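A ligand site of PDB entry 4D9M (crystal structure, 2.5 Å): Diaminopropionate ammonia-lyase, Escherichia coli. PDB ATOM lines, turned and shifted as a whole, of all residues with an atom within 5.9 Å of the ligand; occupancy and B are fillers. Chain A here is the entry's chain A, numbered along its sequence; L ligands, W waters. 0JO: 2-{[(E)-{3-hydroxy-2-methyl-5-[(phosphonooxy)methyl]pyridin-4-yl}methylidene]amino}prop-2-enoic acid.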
ATOM      1  N   ALA A  75      17.388  -6.335  -8.447  1.00  0.00           N
ATOM      2  CA  ALA A  75      17.457  -7.751  -8.071  1.00  0.00           C
ATOM      3  C   ALA A  75      18.396  -8.525  -9.017  1.00  0.00           C
ATOM      4  O   ALA A  75      18.835  -8.000 -10.039  1.00  0.00           O
ATOM      5  CB  ALA A  75      16.063  -8.378  -8.070  1.00  0.00           C
ATOM      6  N   PHE A  76      18.689  -9.767  -8.652  1.00  0.00           N
ATOM      7  CA  PHE A  76      19.634 -10.600  -9.397  1.00  0.00           C
ATOM      8  C   PHE A  76      18.977 -11.393 -10.526  1.00  0.00           C
ATOM      9  O   PHE A  76      19.658 -11.808 -11.468  1.00  0.00           O
ATOM     10  CB  PHE A  76      20.333 -11.590  -8.462  1.00  0.00           C
ATOM     11  CG  PHE A  76      19.509 -12.818  -8.154  1.00  0.00           C
ATOM     12  CD1 PHE A  76      18.432 -12.750  -7.275  1.00  0.00           C
ATOM     13  CD2 PHE A  76      19.807 -14.037  -8.763  1.00  0.00           C
ATOM     14  CE1 PHE A  76      17.673 -13.870  -7.014  1.00  0.00           C
ATOM     15  CE2 PHE A  76      19.053 -15.161  -8.494  1.00  0.00           C
ATOM     16  CZ  PHE A  76      17.984 -15.081  -7.614  1.00  0.00           C
ATOM     17  N   LYS A  77      17.671 -11.617 -10.414  1.00  0.00           N
ATOM     18  CA  LYS A  77      16.939 -12.560 -11.269  1.00  0.00           C
ATOM     19  C   LYS A  77      17.230 -12.384 -12.753  1.00  0.00           C
ATOM     20  O   LYS A  77      17.360 -13.368 -13.487  1.00  0.00           O
ATOM     21  CB  LYS A  77      15.436 -12.471 -10.999  1.00  0.00           C
ATOM     22  CG  LYS A  77      14.972 -13.284  -9.783  1.00  0.00           C
ATOM     23  CD  LYS A  77      14.846 -14.758 -10.137  1.00  0.00           C
ATOM     24  CE  LYS A  77      14.563 -15.624  -8.910  1.00  0.00           C
ATOM     25  NZ  LYS A  77      14.545 -17.090  -9.256  1.00  0.00           N
ATOM     26  N   THR A 118       5.054 -16.903 -14.595  1.00  0.00           N
ATOM     27  CA  THR A 118       4.459 -16.471 -13.332  1.00  0.00           C
ATOM     28  C   THR A 118       5.570 -16.014 -12.388  1.00  0.00           C
ATOM     29  O   THR A 118       6.623 -16.655 -12.285  1.00  0.00           O
ATOM     30  CB  THR A 118       3.617 -17.586 -12.669  1.00  0.00           C
ATOM     31  OG1 THR A 118       2.563 -17.968 -13.561  1.00  0.00           O
ATOM     32  CG2 THR A 118       2.996 -17.116 -11.358  1.00  0.00           C
ATOM     33  N   THR A 119       5.334 -14.895 -11.709  1.00  0.00           N
ATOM     34  CA  THR A 119       6.278 -14.346 -10.744  1.00  0.00           C
ATOM     35  C   THR A 119       5.565 -13.591  -9.626  1.00  0.00           C
ATOM     36  O   THR A 119       4.507 -12.993  -9.842  1.00  0.00           O
ATOM     37  CB  THR A 119       7.318 -13.417 -11.417  1.00  0.00           C
ATOM     38  OG1 THR A 119       8.426 -13.213 -10.533  1.00  0.00           O
ATOM     39  CG2 THR A 119       6.697 -12.054 -11.773  1.00  0.00           C
ATOM     40  N   ASP A 120       6.154 -13.626  -8.428  1.00  0.00           N
ATOM     41  CA  ASP A 120       5.680 -12.785  -7.336  1.00  0.00           C
ATOM     42  C   ASP A 120       6.505 -11.495  -7.268  1.00  0.00           C
ATOM     43  O   ASP A 120       6.362 -10.707  -6.313  1.00  0.00           O
ATOM     44  CB  ASP A 120       5.679 -13.544  -6.009  1.00  0.00           C
ATOM     45  CG  ASP A 120       7.039 -14.116  -5.648  1.00  0.00           C
ATOM     46  OD1 ASP A 120       7.115 -15.329  -5.382  1.00  0.00           O
ATOM     47  OD2 ASP A 120       8.027 -13.347  -5.638  1.00  0.00           O
ATOM     48  N   GLY A 121       7.347 -11.273  -8.267  1.00  0.00           N
ATOM     49  CA  GLY A 121       8.113 -10.030  -8.374  1.00  0.00           C
ATOM     50  C   GLY A 121       9.297  -9.997  -9.338  1.00  0.00           C
ATOM     51  O   GLY A 121       9.186  -9.493 -10.451  1.00  0.00           O
ATOM     52  N   ASN A 122      10.429 -10.521  -8.896  1.00  0.00           N
ATOM     53  CA  ASN A 122      11.713 -10.275  -9.571  1.00  0.00           C
ATOM     54  C   ASN A 122      11.931 -10.998 -10.888  1.00  0.00           C
ATOM     55  O   ASN A 122      12.417 -10.393 -11.847  1.00  0.00           O
ATOM     56  CB  ASN A 122      12.878 -10.551  -8.618  1.00  0.00           C
ATOM     57  CG  ASN A 122      12.917  -9.590  -7.452  1.00  0.00           C
ATOM     58  OD1 ASN A 122      12.667  -8.398  -7.610  1.00  0.00           O
ATOM     59  ND2 ASN A 122      13.241 -10.097  -6.276  1.00  0.00           N
ATOM     60  N   HIS A 123      11.588 -12.286 -10.942  1.00  0.00           N
ATOM     61  CA  HIS A 123      11.826 -13.121 -12.120  1.00  0.00           C
ATOM     62  C   HIS A 123      11.124 -12.605 -13.356  1.00  0.00           C
ATOM     63  O   HIS A 123      11.711 -12.608 -14.444  1.00  0.00           O
ATOM     64  CB  HIS A 123      11.440 -14.572 -11.847  1.00  0.00           C
ATOM     65  CG  HIS A 123      11.446 -15.441 -13.086  1.00  0.00           C
ATOM     66  ND1 HIS A 123      12.579 -15.842 -13.690  1.00  0.00           N
ATOM     67  CD2 HIS A 123      10.397 -15.979 -13.830  1.00  0.00           C
ATOM     68  CE1 HIS A 123      12.272 -16.587 -14.770  1.00  0.00           C
ATOM     69  NE2 HIS A 123      10.937 -16.677 -14.845  1.00  0.00           N
ATOM     70  N   GLY A 124       9.879 -12.180 -13.184  1.00  0.00           N
ATOM     71  CA  GLY A 124       9.076 -11.611 -14.275  1.00  0.00           C
ATOM     72  C   GLY A 124       9.609 -10.274 -14.743  1.00  0.00           C
ATOM     73  O   GLY A 124       9.557  -9.960 -15.933  1.00  0.00           O
ATOM     74  N   ASP A 189      11.072 -20.059 -14.012  1.00  0.00           N
ATOM     75  CA  ASP A 189      12.297 -20.309 -13.248  1.00  0.00           C
ATOM     76  C   ASP A 189      12.330 -21.623 -12.467  1.00  0.00           C
ATOM     77  O   ASP A 189      13.276 -21.879 -11.720  1.00  0.00           O
ATOM     78  CB  ASP A 189      12.649 -19.118 -12.340  1.00  0.00           C
ATOM     79  CG  ASP A 189      11.506 -18.690 -11.433  1.00  0.00           C
ATOM     80  OD1 ASP A 189      10.396 -19.247 -11.519  1.00  0.00           O
ATOM     81  OD2 ASP A 189      11.720 -17.773 -10.610  1.00  0.00           O
ATOM     82  N   TYR A 206      22.455 -17.502 -13.461  1.00  0.00           N
ATOM     83  CA  TYR A 206      22.626 -16.987 -12.101  1.00  0.00           C
ATOM     84  C   TYR A 206      24.065 -16.998 -11.642  1.00  0.00           C
ATOM     85  O   TYR A 206      24.499 -16.103 -10.919  1.00  0.00           O
ATOM     86  CB  TYR A 206      21.790 -17.785 -11.090  1.00  0.00           C
ATOM     87  CG  TYR A 206      20.293 -17.615 -11.189  1.00  0.00           C
ATOM     88  CD1 TYR A 206      19.713 -16.493 -11.791  1.00  0.00           C
ATOM     89  CD2 TYR A 206      19.445 -18.579 -10.633  1.00  0.00           C
ATOM     90  CE1 TYR A 206      18.341 -16.344 -11.872  1.00  0.00           C
ATOM     91  CE2 TYR A 206      18.069 -18.438 -10.703  1.00  0.00           C
ATOM     92  CZ  TYR A 206      17.529 -17.324 -11.327  1.00  0.00           C
ATOM     93  OH  TYR A 206      16.167 -17.193 -11.401  1.00  0.00           O
ATOM     94  N   GLN A 230      19.607 -18.185   0.478  1.00  0.00           N
ATOM     95  CA  GLN A 230      18.155 -18.229   0.628  1.00  0.00           C
ATOM     96  C   GLN A 230      17.564 -19.100  -0.477  1.00  0.00           C
ATOM     97  O   GLN A 230      18.122 -19.178  -1.565  1.00  0.00           O
ATOM     98  CB  GLN A 230      17.519 -16.827   0.645  1.00  0.00           C
ATOM     99  CG  GLN A 230      17.907 -15.876  -0.474  1.00  0.00           C
ATOM    100  CD  GLN A 230      19.182 -15.107  -0.181  1.00  0.00           C
ATOM    101  OE1 GLN A 230      20.275 -15.689  -0.140  1.00  0.00           O
ATOM    102  NE2 GLN A 230      19.055 -13.808   0.031  1.00  0.00           N
ATOM    103  N   ALA A 231      16.457 -19.764  -0.175  1.00  0.00           N
ATOM    104  CA  ALA A 231      15.827 -20.641  -1.152  1.00  0.00           C
ATOM    105  C   ALA A 231      14.309 -20.453  -1.208  1.00  0.00           C
ATOM    106  O   ALA A 231      13.653 -20.368  -0.168  1.00  0.00           O
ATOM    107  CB  ALA A 231      16.165 -22.088  -0.878  1.00  0.00           C
ATOM    108  N   GLY A 232      13.790 -20.351  -2.427  1.00  0.00           N
ATOM    109  CA  GLY A 232      12.351 -20.430  -2.675  1.00  0.00           C
ATOM    110  C   GLY A 232      12.073 -21.797  -3.269  1.00  0.00           C
ATOM    111  O   GLY A 232      11.739 -22.733  -2.545  1.00  0.00           O
ATOM    112  N   VAL A 233      12.215 -21.911  -4.593  1.00  0.00           N
ATOM    113  CA  VAL A 233      12.206 -23.219  -5.242  1.00  0.00           C
ATOM    114  C   VAL A 233      13.615 -23.833  -5.283  1.00  0.00           C
ATOM    115  O   VAL A 233      13.768 -25.018  -5.567  1.00  0.00           O
ATOM    116  CB  VAL A 233      11.618 -23.188  -6.675  1.00  0.00           C
ATOM    117  CG1 VAL A 233      10.163 -22.712  -6.666  1.00  0.00           C
ATOM    118  CG2 VAL A 233      12.468 -22.339  -7.618  1.00  0.00           C
ATOM    119  N   GLY A 234      14.632 -23.007  -5.009  1.00  0.00           N
ATOM    120  CA  GLY A 234      16.018 -23.469  -4.954  1.00  0.00           C
ATOM    121  C   GLY A 234      16.813 -23.383  -6.244  1.00  0.00           C
ATOM    122  O   GLY A 234      17.853 -24.041  -6.390  1.00  0.00           O
ATOM    123  N   ALA A 235      16.343 -22.557  -7.184  1.00  0.00           N
ATOM    124  CA  ALA A 235      17.026 -22.357  -8.465  1.00  0.00           C
ATOM    125  C   ALA A 235      18.335 -21.584  -8.312  1.00  0.00           C
ATOM    126  O   ALA A 235      19.349 -21.959  -8.921  1.00  0.00           O
ATOM    127  CB  ALA A 235      16.104 -21.695  -9.484  1.00  0.00           C
ATOM    128  N   MET A 236      18.311 -20.519  -7.517  1.00  0.00           N
ATOM    129  CA  MET A 236      19.519 -19.738  -7.206  1.00  0.00           C
ATOM    130  C   MET A 236      20.481 -20.542  -6.333  1.00  0.00           C
ATOM    131  O   MET A 236      21.672 -20.646  -6.644  1.00  0.00           O
ATOM    132  CB  MET A 236      19.165 -18.422  -6.514  1.00  0.00           C
ATOM    133  CG  MET A 236      20.364 -17.499  -6.299  1.00  0.00           C
ATOM    134  SD  MET A 236      21.369 -17.818  -4.830  1.00  0.00           S
ATOM    135  CE  MET A 236      20.210 -17.426  -3.514  1.00  0.00           C
ATOM    136  N   ALA A 237      19.966 -21.101  -5.232  1.00  0.00           N
ATOM    137  CA  ALA A 237      20.773 -21.924  -4.352  1.00  0.00           C
ATOM    138  C   ALA A 237      21.500 -23.004  -5.157  1.00  0.00           C
ATOM    139  O   ALA A 237      22.714 -23.135  -5.069  1.00  0.00           O
ATOM    140  CB  ALA A 237      19.920 -22.538  -3.256  1.00  0.00           C
ATOM    141  N   ILE A 266      12.403 -27.179   0.842  1.00  0.00           N
ATOM    142  CA  ILE A 266      13.716 -27.808   0.648  1.00  0.00           C
ATOM    143  C   ILE A 266      14.251 -28.406   1.958  1.00  0.00           C
ATOM    144  O   ILE A 266      14.840 -29.488   1.957  1.00  0.00           O
ATOM    145  CB  ILE A 266      14.712 -26.821  -0.021  1.00  0.00           C
ATOM    146  CG1 ILE A 266      14.368 -26.695  -1.508  1.00  0.00           C
ATOM    147  CG2 ILE A 266      16.159 -27.278   0.133  1.00  0.00           C
ATOM    148  CD1 ILE A 266      14.800 -25.393  -2.154  1.00  0.00           C
ATOM    149  N   ALA A 287       7.644 -12.670  -0.158  1.00  0.00           N
ATOM    150  CA  ALA A 287       7.540 -12.961  -1.587  1.00  0.00           C
ATOM    151  C   ALA A 287       8.924 -13.236  -2.185  1.00  0.00           C
ATOM    152  O   ALA A 287       9.873 -12.489  -1.941  1.00  0.00           O
ATOM    153  CB  ALA A 287       6.871 -11.803  -2.311  1.00  0.00           C
ATOM    154  N   GLY A 288       9.015 -14.318  -2.956  1.00  0.00           N
ATOM    155  CA  GLY A 288      10.296 -14.735  -3.514  1.00  0.00           C
ATOM    156  C   GLY A 288      10.760 -16.065  -2.953  1.00  0.00           C
ATOM    157  O   GLY A 288      11.412 -16.852  -3.653  1.00  0.00           O
ATOM    158  N   LEU A 289      10.422 -16.327  -1.695  1.00  0.00           N
ATOM    159  CA  LEU A 289      10.862 -17.542  -1.019  1.00  0.00           C
ATOM    160  C   LEU A 289       9.731 -18.563  -0.804  1.00  0.00           C
ATOM    161  O   LEU A 289       9.945 -19.621  -0.218  1.00  0.00           O
ATOM    162  CB  LEU A 289      11.587 -17.208   0.286  1.00  0.00           C
ATOM    163  CG  LEU A 289      12.797 -16.275   0.180  1.00  0.00           C
ATOM    164  CD1 LEU A 289      13.474 -16.089   1.535  1.00  0.00           C
ATOM    165  CD2 LEU A 289      13.808 -16.785  -0.841  1.00  0.00           C
ATOM    166  N   ALA A 290       8.543 -18.221  -1.286  1.00  0.00           N
ATOM    167  CA  ALA A 290       7.404 -19.149  -1.319  1.00  0.00           C
ATOM    168  C   ALA A 290       7.742 -20.341  -2.202  1.00  0.00           C
ATOM    169  O   ALA A 290       8.527 -20.209  -3.147  1.00  0.00           O
ATOM    170  CB  ALA A 290       6.158 -18.447  -1.823  1.00  0.00           C
ATOM    171  N   SER A 339      13.212 -11.024   1.067  1.00  0.00           N
ATOM    172  CA  SER A 339      13.854 -12.240   0.553  1.00  0.00           C
ATOM    173  C   SER A 339      15.362 -12.081   0.366  1.00  0.00           C
ATOM    174  O   SER A 339      16.100 -13.066   0.287  1.00  0.00           O
ATOM    175  CB  SER A 339      13.205 -12.681  -0.757  1.00  0.00           C
ATOM    176  OG  SER A 339      11.873 -13.094  -0.538  1.00  0.00           O
ATOM    177  N   GLY A 340      15.830 -10.832   0.309  1.00  0.00           N
ATOM    178  CA  GLY A 340      17.243 -10.548   0.081  1.00  0.00           C
ATOM    179  C   GLY A 340      18.108 -10.621   1.325  1.00  0.00           C
ATOM    180  O   GLY A 340      19.306 -10.899   1.221  1.00  0.00           O
ATOM    181  N   THR A 376      19.950 -10.770  -2.359  1.00  0.00           N
ATOM    182  CA  THR A 376      19.377 -11.100  -3.665  1.00  0.00           C
ATOM    183  C   THR A 376      18.517  -9.985  -4.284  1.00  0.00           C
ATOM    184  O   THR A 376      18.281  -9.975  -5.486  1.00  0.00           O
ATOM    185  CB  THR A 376      18.594 -12.433  -3.638  1.00  0.00           C
ATOM    186  OG1 THR A 376      17.725 -12.455  -2.491  1.00  0.00           O
ATOM    187  CG2 THR A 376      19.535 -13.620  -3.567  1.00  0.00           C
ATOM    188  N   GLU A 377      18.052  -9.053  -3.455  1.00  0.00           N
ATOM    189  CA  GLU A 377      17.265  -7.924  -3.919  1.00  0.00           C
ATOM    190  C   GLU A 377      17.421  -6.703  -3.025  1.00  0.00           C
ATOM    191  O   GLU A 377      17.825  -6.820  -1.856  1.00  0.00           O
ATOM    192  CB  GLU A 377      15.772  -8.292  -4.006  1.00  0.00           C
ATOM    193  CG  GLU A 377      15.059  -8.384  -2.654  1.00  0.00           C
ATOM    194  CD  GLU A 377      13.563  -8.648  -2.783  1.00  0.00           C
ATOM    195  OE1 GLU A 377      13.025  -8.625  -3.912  1.00  0.00           O
ATOM    196  OE2 GLU A 377      12.914  -8.892  -1.748  1.00  0.00           O
HETATM  197  O   0JO L   1       9.215 -14.979  -8.876  1.00  0.00           O
HETATM  198  C   0JO L   1      10.300 -14.755  -8.278  1.00  0.00           C
HETATM  199  OXT 0JO L   1      11.058 -13.838  -8.652  1.00  0.00           O
HETATM  200  CA  0JO L   1      10.664 -15.569  -7.118  1.00  0.00           C
HETATM  201  CB  0JO L   1      10.074 -16.723  -6.854  1.00  0.00           C
HETATM  202  N   0JO L   1      11.603 -15.096  -6.289  1.00  0.00           N
HETATM  203  C4A 0JO L   1      12.787 -15.560  -6.237  1.00  0.00           C
HETATM  204  C4  0JO L   1      13.789 -14.981  -5.296  1.00  0.00           C
HETATM  205  C3  0JO L   1      13.983 -13.607  -5.211  1.00  0.00           C
HETATM  206  O3  0JO L   1      13.253 -12.749  -5.982  1.00  0.00           O
HETATM  207  C2  0JO L   1      14.929 -13.111  -4.328  1.00  0.00           C
HETATM  208  C2A 0JO L   1      15.152 -11.622  -4.214  1.00  0.00           C
HETATM  209  N1  0JO L   1      15.669 -13.933  -3.555  1.00  0.00           N
HETATM  210  C6  0JO L   1      15.513 -15.250  -3.615  1.00  0.00           C
HETATM  211  C5  0JO L   1      14.573 -15.805  -4.485  1.00  0.00           C
HETATM  212  C5A 0JO L   1      14.424 -17.300  -4.503  1.00  0.00           C
HETATM  213  OP4 0JO L   1      15.100 -17.870  -5.621  1.00  0.00           O
HETATM  214  P   0JO L   1      14.740 -19.379  -6.020  1.00  0.00           P
HETATM  215  OP3 0JO L   1      13.258 -19.375  -6.334  1.00  0.00           O
HETATM  216  OP1 0JO L   1      15.688 -19.564  -7.169  1.00  0.00           O
HETATM  217  OP2 0JO L   1      15.047 -20.206  -4.793  1.00  0.00           O
HETATM  218  O   HOH W   1      17.438 -20.319  -4.179  1.00  0.00           O
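Water W1 lies within hydrogen-bond range of an oxygen (OP2) of the ligand, the backbone NH (N) of Ala 237, the backbone carbonyl oxygen (O) of Gln 230 and the backbone NH (N) of Met 236.
The backbone NH (N) of Gly 232 lies within hydrogen-bond range of an oxygen (OP2) of the ligand, at 2.7 Å. The side-chain hydroxyl (OG1) of Thr 119 is in hydrogen-bond range of an oxygen (O) of the ligand (2.5 Å). The backbone NH (N) of Gly 234 sits at hydrogen-bond distance from an oxygen (OP2) of the ligand, at 2.8 Å. The backbone NH (N) of Asn 122 sits at hydrogen-bond distance from an oxygen (OXT) of the ligand. The backbone NH (N) of Met 236 is in hydrogen-bond range of an oxygen (OP1) of the ligand, at 2.8 Å. The backbone NH (N) of His 123 sits at hydrogen-bond distance from an oxygen (OXT) of the ligand (2.8 Å). The backbone NH (N) of Asp 120 is in hydrogen-bond range of an oxygen (O) of the ligand (3.4 Å). The side-chain amide nitrogen (ND2) of Asn 122 is in hydrogen-bond range of an oxygen (O3) of the ligand, at 2.7 Å. An oxygen (OP3) of the ligand lies within hydrogen-bond range of the backbone NH (N) of Val 233 (3.2 Å). The backbone NH of Ala 235 is in hydrogen-bond range of an oxygen (OP1) of the ligand (3.1 Å). The side-chain hydroxyl of Thr 376 sits at hydrogen-bond distance from a nitrogen (N1) of the ligand (2.7 Å). OP1 of the ligand lies within salt-bridge range of NZ of Lys 77.
O of Ser 339 lies within hydrogen-bond range of OG1 of Thr 376 (3.3 Å). The backbone NH of Gly 121 is in hydrogen-bond range of the side-chain hydroxyl of Thr 119, at 3.2 Å. OG of Ser 339 sits at hydrogen-bond distance from O of Ala 287 (2.5 Å). The side-chain amino group (NZ) of Lys 77 sits at hydrogen-bond distance from the side-chain hydroxyl (OH) of Tyr 206. The backbone NH (N) of Gly 124 sits at hydrogen-bond distance from the side-chain hydroxyl (OG1) of Thr 119 (3.2 Å). The side-chain amide nitrogen (ND2) of Asn 122 lies within hydrogen-bond range of the side-chain carboxylate (OE1) of Glu 377, 2.8 Å away. OG1 of Thr 119 sits at hydrogen-bond distance from N of His 123 (3.3 Å). The backbone NH of Gly 288 sits at hydrogen-bond distance from the side-chain carboxylate of Asp 120.
The backbone carbonyl oxygen of Gly 288 lies close to a nitrogen (N) of the ligand (3.2 Å). Residues that only touch the ligand: Phe 76 (3.9 Å), Gln 230 (3.999 Å), Ala 231 (3.7 Å), Leu 289 (3.6 Å), Ser 339 (3.9 Å) and Glu 377 (3.4 Å). Hydrophobic or aromatic side chains within 4 Å of the ligand: Phe 76, His 123, Val 233, Ala 235, Met 236 and Leu 289. 18 residues have an atom within 4 Å of the ligand: Phe 76, Lys 77, Thr 119, Asp 120, Asn 122, His 123, Gln 230, Ala 231, Gly 232, Val 233, Gly 234, Ala 235, Met 236, Gly 288, Leu 289, Ser 339, Thr 376 and Glu 377. The nearest printed residue that does not touch the ligand is Asp 189 (4.1 Å).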
